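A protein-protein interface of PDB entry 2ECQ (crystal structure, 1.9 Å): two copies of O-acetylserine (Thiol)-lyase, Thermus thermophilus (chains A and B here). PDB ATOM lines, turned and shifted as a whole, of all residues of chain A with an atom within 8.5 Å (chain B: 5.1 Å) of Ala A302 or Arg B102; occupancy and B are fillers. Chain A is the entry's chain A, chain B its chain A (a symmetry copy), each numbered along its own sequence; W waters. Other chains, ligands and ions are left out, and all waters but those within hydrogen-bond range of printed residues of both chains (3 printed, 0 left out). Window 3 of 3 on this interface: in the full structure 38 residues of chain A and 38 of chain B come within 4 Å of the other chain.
The guanidinium group (NH1) of Arg B102 sits at hydrogen-bond distance from the backbone carbonyl oxygen (O) of Leu A296 (2.9 Å).
O of Phe A259 sits at hydrogen-bond distance from N of Gly A292 (3.0 Å).
Ala A253 touches Ala B106. Phe A259 touches Ala B106. Leu A296 touches Glu B99 (CD1 to CG, 3.6 Å). Val B103 touches Leu A296 (CG2 to CD1, 3.2 Å). Ser A297 touches Arg B102. CG of Arg B102 touches O of Tyr A301 (3.8 Å). Ala B106 touches Tyr A301. Ala A302 touches Arg B102.
Printed residues of chain B within 4 Å of Phe A259: Ala B106. Ala A302 touches just one residue of chain B: Arg B102 (3.9 Å). Of the printed residues of chain A, Glu B99 touches Leu A296 (3.6 Å). Lys B101 touches none of the printed residues of chain A. Arg B102 touches four residues of chain A.
Printed residues of chain A that touch a printed residue of chain B: Ala A253, Phe A259, Leu A296, Ser A297, Tyr A301 and Ala A302. Among the printed residues, 9 pairs touch across the chains. Among the printed residues, no Asp or Glu carboxylate lies within 4 Å of a Lys or Arg side-chain nitrogen of the other chain.
Position printed for both chains: 99. Of the 9 pairs that touch across the chains among the printed residues, none has its exchanged pair printed and touching as well.
Water W2 lies within hydrogen-bond range of O of Ala B106 (2.7 Å) and O of Arg A250 (2.9 Å). Water W1 lies within hydrogen-bond range of the guanidinium group of Arg B102 (2.7 Å) and the side-chain hydroxyl of Ser A297 (3.5 Å). Water W3 bridges the backbone carbonyl oxygen of Tyr A301 (2.8 Å) and the backbone carbonyl oxygen of Arg B102 (2.9 Å).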
ATOM      1  N   GLU A  99     -28.142  22.269   5.844  1.00  0.00           N
ATOM      2  CA  GLU A  99     -28.457  21.632   4.571  1.00  0.00           C
ATOM      3  C   GLU A  99     -27.748  20.281   4.446  1.00  0.00           C
ATOM      4  O   GLU A  99     -28.378  19.262   4.146  1.00  0.00           O
ATOM      5  CB  GLU A  99     -28.040  22.540   3.411  1.00  0.00           C
ATOM      6  CG  GLU A  99     -28.610  22.120   2.067  1.00  0.00           C
ATOM      7  CD  GLU A  99     -28.070  22.951   0.919  1.00  0.00           C
ATOM      8  OE1 GLU A  99     -27.782  24.147   1.138  1.00  0.00           O
ATOM      9  OE2 GLU A  99     -27.946  22.412  -0.200  1.00  0.00           O
ATOM     10  N   PHE A 246     -14.940  30.104 -10.248  1.00  0.00           N
ATOM     11  CA  PHE A 246     -16.367  30.304 -10.039  1.00  0.00           C
ATOM     12  C   PHE A 246     -17.034  30.940 -11.258  1.00  0.00           C
ATOM     13  O   PHE A 246     -18.108  30.504 -11.673  1.00  0.00           O
ATOM     14  CB  PHE A 246     -16.595  31.119  -8.762  1.00  0.00           C
ATOM     15  CG  PHE A 246     -16.354  30.330  -7.493  1.00  0.00           C
ATOM     16  CD1 PHE A 246     -15.510  29.217  -7.493  1.00  0.00           C
ATOM     17  CD2 PHE A 246     -16.954  30.708  -6.295  1.00  0.00           C
ATOM     18  CE1 PHE A 246     -15.269  28.495  -6.319  1.00  0.00           C
ATOM     19  CE2 PHE A 246     -16.718  29.995  -5.114  1.00  0.00           C
ATOM     20  CZ  PHE A 246     -15.874  28.885  -5.128  1.00  0.00           C
ATOM     21  N   ARG A 250     -19.953  29.204 -13.720  1.00  0.00           N
ATOM     22  CA  ARG A 250     -21.200  29.835 -14.118  1.00  0.00           C
ATOM     23  C   ARG A 250     -21.318  29.834 -15.644  1.00  0.00           C
ATOM     24  O   ARG A 250     -22.413  29.679 -16.184  1.00  0.00           O
ATOM     25  CB  ARG A 250     -21.287  31.255 -13.543  1.00  0.00           C
ATOM     26  CG  ARG A 250     -21.478  31.274 -12.022  1.00  0.00           C
ATOM     27  CD  ARG A 250     -21.844  32.659 -11.494  1.00  0.00           C
ATOM     28  NE  ARG A 250     -20.710  33.579 -11.467  1.00  0.00           N
ATOM     29  CZ  ARG A 250     -19.839  33.669 -10.464  1.00  0.00           C
ATOM     30  NH1 ARG A 250     -19.964  32.895  -9.392  1.00  0.00           N
ATOM     31  NH2 ARG A 250     -18.845  34.543 -10.532  1.00  0.00           N
ATOM     32  N   ALA A 253     -22.468  26.448 -16.872  1.00  0.00           N
ATOM     33  CA  ALA A 253     -23.895  26.257 -16.665  1.00  0.00           C
ATOM     34  C   ALA A 253     -24.720  26.987 -17.722  1.00  0.00           C
ATOM     35  O   ALA A 253     -25.620  26.398 -18.325  1.00  0.00           O
ATOM     36  CB  ALA A 253     -24.287  26.732 -15.270  1.00  0.00           C
ATOM     37  N   PHE A 259     -24.322  22.272 -15.123  1.00  0.00           N
ATOM     38  CA  PHE A 259     -24.469  22.847 -13.786  1.00  0.00           C
ATOM     39  C   PHE A 259     -23.632  21.979 -12.849  1.00  0.00           C
ATOM     40  O   PHE A 259     -24.111  20.969 -12.331  1.00  0.00           O
ATOM     41  CB  PHE A 259     -25.958  22.803 -13.414  1.00  0.00           C
ATOM     42  CG  PHE A 259     -26.285  23.356 -12.055  1.00  0.00           C
ATOM     43  CD1 PHE A 259     -25.898  24.640 -11.693  1.00  0.00           C
ATOM     44  CD2 PHE A 259     -27.044  22.606 -11.162  1.00  0.00           C
ATOM     45  CE1 PHE A 259     -26.266  25.171 -10.461  1.00  0.00           C
ATOM     46  CE2 PHE A 259     -27.418  23.129  -9.926  1.00  0.00           C
ATOM     47  CZ  PHE A 259     -27.030  24.413  -9.575  1.00  0.00           C
ATOM     48  N   MET A 262     -18.360  23.270  -7.193  1.00  0.00           N
ATOM     49  CA  MET A 262     -17.247  24.186  -7.015  1.00  0.00           C
ATOM     50  C   MET A 262     -15.912  23.599  -7.489  1.00  0.00           C
ATOM     51  O   MET A 262     -15.160  24.261  -8.206  1.00  0.00           O
ATOM     52  CB  MET A 262     -17.190  24.594  -5.539  1.00  0.00           C
ATOM     53  CG  MET A 262     -18.589  24.940  -4.979  1.00  0.00           C
ATOM     54  SD  MET A 262     -18.617  25.352  -3.234  1.00  0.00           S
ATOM     55  CE  MET A 262     -18.684  27.152  -3.308  1.00  0.00           C
ATOM     56  N   GLY A 292     -24.025  20.999  -9.355  1.00  0.00           N
ATOM     57  CA  GLY A 292     -24.200  22.196  -8.556  1.00  0.00           C
ATOM     58  C   GLY A 292     -25.323  22.136  -7.536  1.00  0.00           C
ATOM     59  O   GLY A 292     -25.469  23.055  -6.731  1.00  0.00           O
ATOM     60  N   TRP A 293     -26.093  21.050  -7.550  1.00  0.00           N
ATOM     61  CA  TRP A 293     -27.242  20.885  -6.659  1.00  0.00           C
ATOM     62  C   TRP A 293     -27.046  21.157  -5.168  1.00  0.00           C
ATOM     63  O   TRP A 293     -27.935  21.709  -4.521  1.00  0.00           O
ATOM     64  CB  TRP A 293     -27.842  19.488  -6.848  1.00  0.00           C
ATOM     65  CG  TRP A 293     -28.131  19.205  -8.279  1.00  0.00           C
ATOM     66  CD1 TRP A 293     -27.365  18.477  -9.143  1.00  0.00           C
ATOM     67  CD2 TRP A 293     -29.210  19.742  -9.053  1.00  0.00           C
ATOM     68  NE1 TRP A 293     -27.897  18.533 -10.410  1.00  0.00           N
ATOM     69  CE2 TRP A 293     -29.029  19.303 -10.383  1.00  0.00           C
ATOM     70  CE3 TRP A 293     -30.310  20.557  -8.753  1.00  0.00           C
ATOM     71  CZ2 TRP A 293     -29.908  19.652 -11.414  1.00  0.00           C
ATOM     72  CZ3 TRP A 293     -31.187  20.903  -9.779  1.00  0.00           C
ATOM     73  CH2 TRP A 293     -30.977  20.451 -11.092  1.00  0.00           C
ATOM     74  N   TYR A 295     -24.866  23.197  -3.931  1.00  0.00           N
ATOM     75  CA  TYR A 295     -24.232  24.490  -3.707  1.00  0.00           C
ATOM     76  C   TYR A 295     -25.013  25.757  -4.041  1.00  0.00           C
ATOM     77  O   TYR A 295     -24.418  26.796  -4.324  1.00  0.00           O
ATOM     78  CB  TYR A 295     -22.893  24.505  -4.444  1.00  0.00           C
ATOM     79  CG  TYR A 295     -22.091  23.240  -4.224  1.00  0.00           C
ATOM     80  CD1 TYR A 295     -22.098  22.208  -5.167  1.00  0.00           C
ATOM     81  CD2 TYR A 295     -21.346  23.064  -3.059  1.00  0.00           C
ATOM     82  CE1 TYR A 295     -21.374  21.028  -4.952  1.00  0.00           C
ATOM     83  CE2 TYR A 295     -20.624  21.891  -2.831  1.00  0.00           C
ATOM     84  CZ  TYR A 295     -20.641  20.881  -3.778  1.00  0.00           C
ATOM     85  OH  TYR A 295     -19.914  19.735  -3.548  1.00  0.00           O
ATOM     86  N   LEU A 296     -26.335  25.690  -3.982  1.00  0.00           N
ATOM     87  CA  LEU A 296     -27.150  26.860  -4.291  1.00  0.00           C
ATOM     88  C   LEU A 296     -27.058  27.955  -3.227  1.00  0.00           C
ATOM     89  O   LEU A 296     -27.419  29.107  -3.481  1.00  0.00           O
ATOM     90  CB  LEU A 296     -28.605  26.436  -4.490  1.00  0.00           C
ATOM     91  CG  LEU A 296     -28.843  25.608  -5.755  1.00  0.00           C
ATOM     92  CD1 LEU A 296     -30.233  25.012  -5.714  1.00  0.00           C
ATOM     93  CD2 LEU A 296     -28.653  26.488  -6.987  1.00  0.00           C
ATOM     94  N   SER A 297     -26.572  27.601  -2.040  1.00  0.00           N
ATOM     95  CA  SER A 297     -26.433  28.574  -0.961  1.00  0.00           C
ATOM     96  C   SER A 297     -24.981  28.978  -0.744  1.00  0.00           C
ATOM     97  O   SER A 297     -24.604  29.399   0.348  1.00  0.00           O
ATOM     98  CB  SER A 297     -27.006  28.015   0.344  1.00  0.00           C
ATOM     99  OG  SER A 297     -28.413  27.869   0.253  1.00  0.00           O
ATOM    100  N   THR A 298     -24.171  28.847  -1.789  1.00  0.00           N
ATOM    101  CA  THR A 298     -22.762  29.209  -1.718  1.00  0.00           C
ATOM    102  C   THR A 298     -22.529  30.353  -2.693  1.00  0.00           C
ATOM    103  O   THR A 298     -23.356  30.606  -3.565  1.00  0.00           O
ATOM    104  CB  THR A 298     -21.853  28.029  -2.122  1.00  0.00           C
ATOM    105  OG1 THR A 298     -22.021  27.756  -3.520  1.00  0.00           O
ATOM    106  CG2 THR A 298     -22.210  26.782  -1.322  1.00  0.00           C
ATOM    107  N   PRO A 299     -21.398  31.063  -2.559  1.00  0.00           N
ATOM    108  CA  PRO A 299     -21.105  32.178  -3.462  1.00  0.00           C
ATOM    109  C   PRO A 299     -21.040  31.796  -4.939  1.00  0.00           C
ATOM    110  O   PRO A 299     -21.151  32.658  -5.810  1.00  0.00           O
ATOM    111  CB  PRO A 299     -19.774  32.714  -2.932  1.00  0.00           C
ATOM    112  CG  PRO A 299     -19.151  31.515  -2.285  1.00  0.00           C
ATOM    113  CD  PRO A 299     -20.318  30.891  -1.574  1.00  0.00           C
ATOM    114  N   LEU A 300     -20.869  30.509  -5.226  1.00  0.00           N
ATOM    115  CA  LEU A 300     -20.799  30.063  -6.613  1.00  0.00           C
ATOM    116  C   LEU A 300     -22.093  30.366  -7.362  1.00  0.00           C
ATOM    117  O   LEU A 300     -22.059  30.884  -8.474  1.00  0.00           O
ATOM    118  CB  LEU A 300     -20.510  28.560  -6.690  1.00  0.00           C
ATOM    119  CG  LEU A 300     -20.476  27.961  -8.102  1.00  0.00           C
ATOM    120  CD1 LEU A 300     -19.439  28.690  -8.945  1.00  0.00           C
ATOM    121  CD2 LEU A 300     -20.156  26.474  -8.031  1.00  0.00           C
ATOM    122  N   TYR A 301     -23.229  30.050  -6.746  1.00  0.00           N
ATOM    123  CA  TYR A 301     -24.526  30.273  -7.379  1.00  0.00           C
ATOM    124  C   TYR A 301     -25.477  31.209  -6.638  1.00  0.00           C
ATOM    125  O   TYR A 301     -26.575  31.482  -7.123  1.00  0.00           O
ATOM    126  CB  TYR A 301     -25.228  28.930  -7.604  1.00  0.00           C
ATOM    127  CG  TYR A 301     -24.503  28.016  -8.563  1.00  0.00           C
ATOM    128  CD1 TYR A 301     -24.003  26.780  -8.143  1.00  0.00           C
ATOM    129  CD2 TYR A 301     -24.307  28.388  -9.893  1.00  0.00           C
ATOM    130  CE1 TYR A 301     -23.325  25.940  -9.029  1.00  0.00           C
ATOM    131  CE2 TYR A 301     -23.633  27.559 -10.783  1.00  0.00           C
ATOM    132  CZ  TYR A 301     -23.144  26.341 -10.346  1.00  0.00           C
ATOM    133  OH  TYR A 301     -22.463  25.534 -11.228  1.00  0.00           O
ATOM    134  N   ALA A 302     -25.068  31.699  -5.471  1.00  0.00           N
ATOM    135  CA  ALA A 302     -25.921  32.596  -4.698  1.00  0.00           C
ATOM    136  C   ALA A 302     -25.837  34.034  -5.205  1.00  0.00           C
ATOM    137  O   ALA A 302     -24.913  34.340  -5.989  1.00  0.00           O
ATOM    138  CB  ALA A 302     -25.539  32.540  -3.221  1.00  0.00           C
ATOM    139  N   GLU B  98     -36.261  31.357  -3.568  1.00  0.00           N
ATOM    140  CA  GLU B  98     -34.974  31.821  -4.067  1.00  0.00           C
ATOM    141  C   GLU B  98     -34.117  30.660  -4.556  1.00  0.00           C
ATOM    142  O   GLU B  98     -33.371  30.794  -5.523  1.00  0.00           O
ATOM    143  CB  GLU B  98     -34.232  32.587  -2.970  1.00  0.00           C
ATOM    144  CG  GLU B  98     -34.957  33.838  -2.498  1.00  0.00           C
ATOM    145  CD  GLU B  98     -35.178  34.836  -3.619  1.00  0.00           C
ATOM    146  OE1 GLU B  98     -34.178  35.247  -4.249  1.00  0.00           O
ATOM    147  OE2 GLU B  98     -36.346  35.209  -3.869  1.00  0.00           O
ATOM    148  N   GLU B  99     -34.230  29.521  -3.884  1.00  0.00           N
ATOM    149  CA  GLU B  99     -33.463  28.338  -4.252  1.00  0.00           C
ATOM    150  C   GLU B  99     -33.736  27.938  -5.704  1.00  0.00           C
ATOM    151  O   GLU B  99     -32.805  27.749  -6.493  1.00  0.00           O
ATOM    152  CB  GLU B  99     -33.816  27.172  -3.323  1.00  0.00           C
ATOM    153  CG  GLU B  99     -32.850  26.003  -3.412  1.00  0.00           C
ATOM    154  CD  GLU B  99     -33.300  24.811  -2.589  1.00  0.00           C
ATOM    155  OE1 GLU B  99     -33.940  25.025  -1.537  1.00  0.00           O
ATOM    156  OE2 GLU B  99     -33.005  23.666  -2.988  1.00  0.00           O
ATOM    157  N   ARG B 100     -35.013  27.812  -6.050  1.00  0.00           N
ATOM    158  CA  ARG B 100     -35.396  27.432  -7.406  1.00  0.00           C
ATOM    159  C   ARG B 100     -34.980  28.494  -8.420  1.00  0.00           C
ATOM    160  O   ARG B 100     -34.486  28.174  -9.500  1.00  0.00           O
ATOM    161  CB  ARG B 100     -36.906  27.195  -7.485  1.00  0.00           C
ATOM    162  CG  ARG B 100     -37.395  26.730  -8.857  1.00  0.00           C
ATOM    163  CD  ARG B 100     -36.606  25.515  -9.358  1.00  0.00           C
ATOM    164  NE  ARG B 100     -36.700  24.374  -8.446  1.00  0.00           N
ATOM    165  CZ  ARG B 100     -37.779  23.609  -8.306  1.00  0.00           C
ATOM    166  NH1 ARG B 100     -38.868  23.854  -9.023  1.00  0.00           N
ATOM    167  NH2 ARG B 100     -37.774  22.600  -7.442  1.00  0.00           N
ATOM    168  N   LYS B 101     -35.176  29.761  -8.070  1.00  0.00           N
ATOM    169  CA  LYS B 101     -34.794  30.842  -8.963  1.00  0.00           C
ATOM    170  C   LYS B 101     -33.295  30.785  -9.260  1.00  0.00           C
ATOM    171  O   LYS B 101     -32.871  31.047 -10.385  1.00  0.00           O
ATOM    172  CB  LYS B 101     -35.174  32.191  -8.344  1.00  0.00           C
ATOM    173  CG  LYS B 101     -36.678  32.459  -8.373  1.00  0.00           C
ATOM    174  CD  LYS B 101     -37.114  33.457  -7.301  1.00  0.00           C
ATOM    175  CE  LYS B 101     -36.488  34.825  -7.492  1.00  0.00           C
ATOM    176  NZ  LYS B 101     -36.967  35.799  -6.465  1.00  0.00           N
ATOM    177  N   ARG B 102     -32.495  30.426  -8.259  1.00  0.00           N
ATOM    178  CA  ARG B 102     -31.050  30.341  -8.451  1.00  0.00           C
ATOM    179  C   ARG B 102     -30.672  29.228  -9.419  1.00  0.00           C
ATOM    180  O   ARG B 102     -29.727  29.372 -10.196  1.00  0.00           O
ATOM    181  CB  ARG B 102     -30.334  30.128  -7.114  1.00  0.00           C
ATOM    182  CG  ARG B 102     -30.317  31.361  -6.232  1.00  0.00           C
ATOM    183  CD  ARG B 102     -29.693  31.066  -4.882  1.00  0.00           C
ATOM    184  NE  ARG B 102     -29.736  32.233  -4.009  1.00  0.00           N
ATOM    185  CZ  ARG B 102     -29.444  32.208  -2.713  1.00  0.00           C
ATOM    186  NH1 ARG B 102     -29.086  31.070  -2.133  1.00  0.00           N
ATOM    187  NH2 ARG B 102     -29.518  33.322  -1.995  1.00  0.00           N
ATOM    188  N   VAL B 103     -31.401  28.118  -9.371  1.00  0.00           N
ATOM    189  CA  VAL B 103     -31.120  27.005 -10.272  1.00  0.00           C
ATOM    190  C   VAL B 103     -31.406  27.432 -11.709  1.00  0.00           C
ATOM    191  O   VAL B 103     -30.583  27.235 -12.602  1.00  0.00           O
ATOM    192  CB  VAL B 103     -31.995  25.773  -9.943  1.00  0.00           C
ATOM    193  CG1 VAL B 103     -31.775  24.681 -10.985  1.00  0.00           C
ATOM    194  CG2 VAL B 103     -31.649  25.248  -8.563  1.00  0.00           C
ATOM    195  N   LEU B 104     -32.574  28.030 -11.922  1.00  0.00           N
ATOM    196  CA  LEU B 104     -32.960  28.469 -13.257  1.00  0.00           C
ATOM    197  C   LEU B 104     -32.004  29.528 -13.801  1.00  0.00           C
ATOM    198  O   LEU B 104     -31.583  29.452 -14.956  1.00  0.00           O
ATOM    199  CB  LEU B 104     -34.397  29.000 -13.239  1.00  0.00           C
ATOM    200  CG  LEU B 104     -35.443  27.981 -12.773  1.00  0.00           C
ATOM    201  CD1 LEU B 104     -36.797  28.657 -12.614  1.00  0.00           C
ATOM    202  CD2 LEU B 104     -35.535  26.833 -13.783  1.00  0.00           C
ATOM    203  N   LYS B 105     -31.643  30.500 -12.969  1.00  0.00           N
ATOM    204  CA  LYS B 105     -30.729  31.554 -13.399  1.00  0.00           C
ATOM    205  C   LYS B 105     -29.316  31.031 -13.636  1.00  0.00           C
ATOM    206  O   LYS B 105     -28.565  31.603 -14.422  1.00  0.00           O
ATOM    207  CB  LYS B 105     -30.688  32.686 -12.372  1.00  0.00           C
ATOM    208  CG  LYS B 105     -31.985  33.474 -12.276  1.00  0.00           C
ATOM    209  CD  LYS B 105     -31.844  34.638 -11.312  1.00  0.00           C
ATOM    210  CE  LYS B 105     -33.136  35.427 -11.228  1.00  0.00           C
ATOM    211  NZ  LYS B 105     -33.590  35.848 -12.584  1.00  0.00           N
ATOM    212  N   ALA B 106     -28.950  29.953 -12.952  1.00  0.00           N
ATOM    213  CA  ALA B 106     -27.619  29.382 -13.136  1.00  0.00           C
ATOM    214  C   ALA B 106     -27.500  28.906 -14.585  1.00  0.00           C
ATOM    215  O   ALA B 106     -26.440  29.016 -15.208  1.00  0.00           O
ATOM    216  CB  ALA B 106     -27.410  28.219 -12.178  1.00  0.00           C
HETATM  217  O   HOH W   1     -30.786  28.944  -2.048  1.00  0.00           O
HETATM  218  O   HOH W   2     -24.384  30.426 -14.201  1.00  0.00           O
HETATM  219  O   HOH W   3     -27.536  31.278  -9.779  1.00  0.00           O
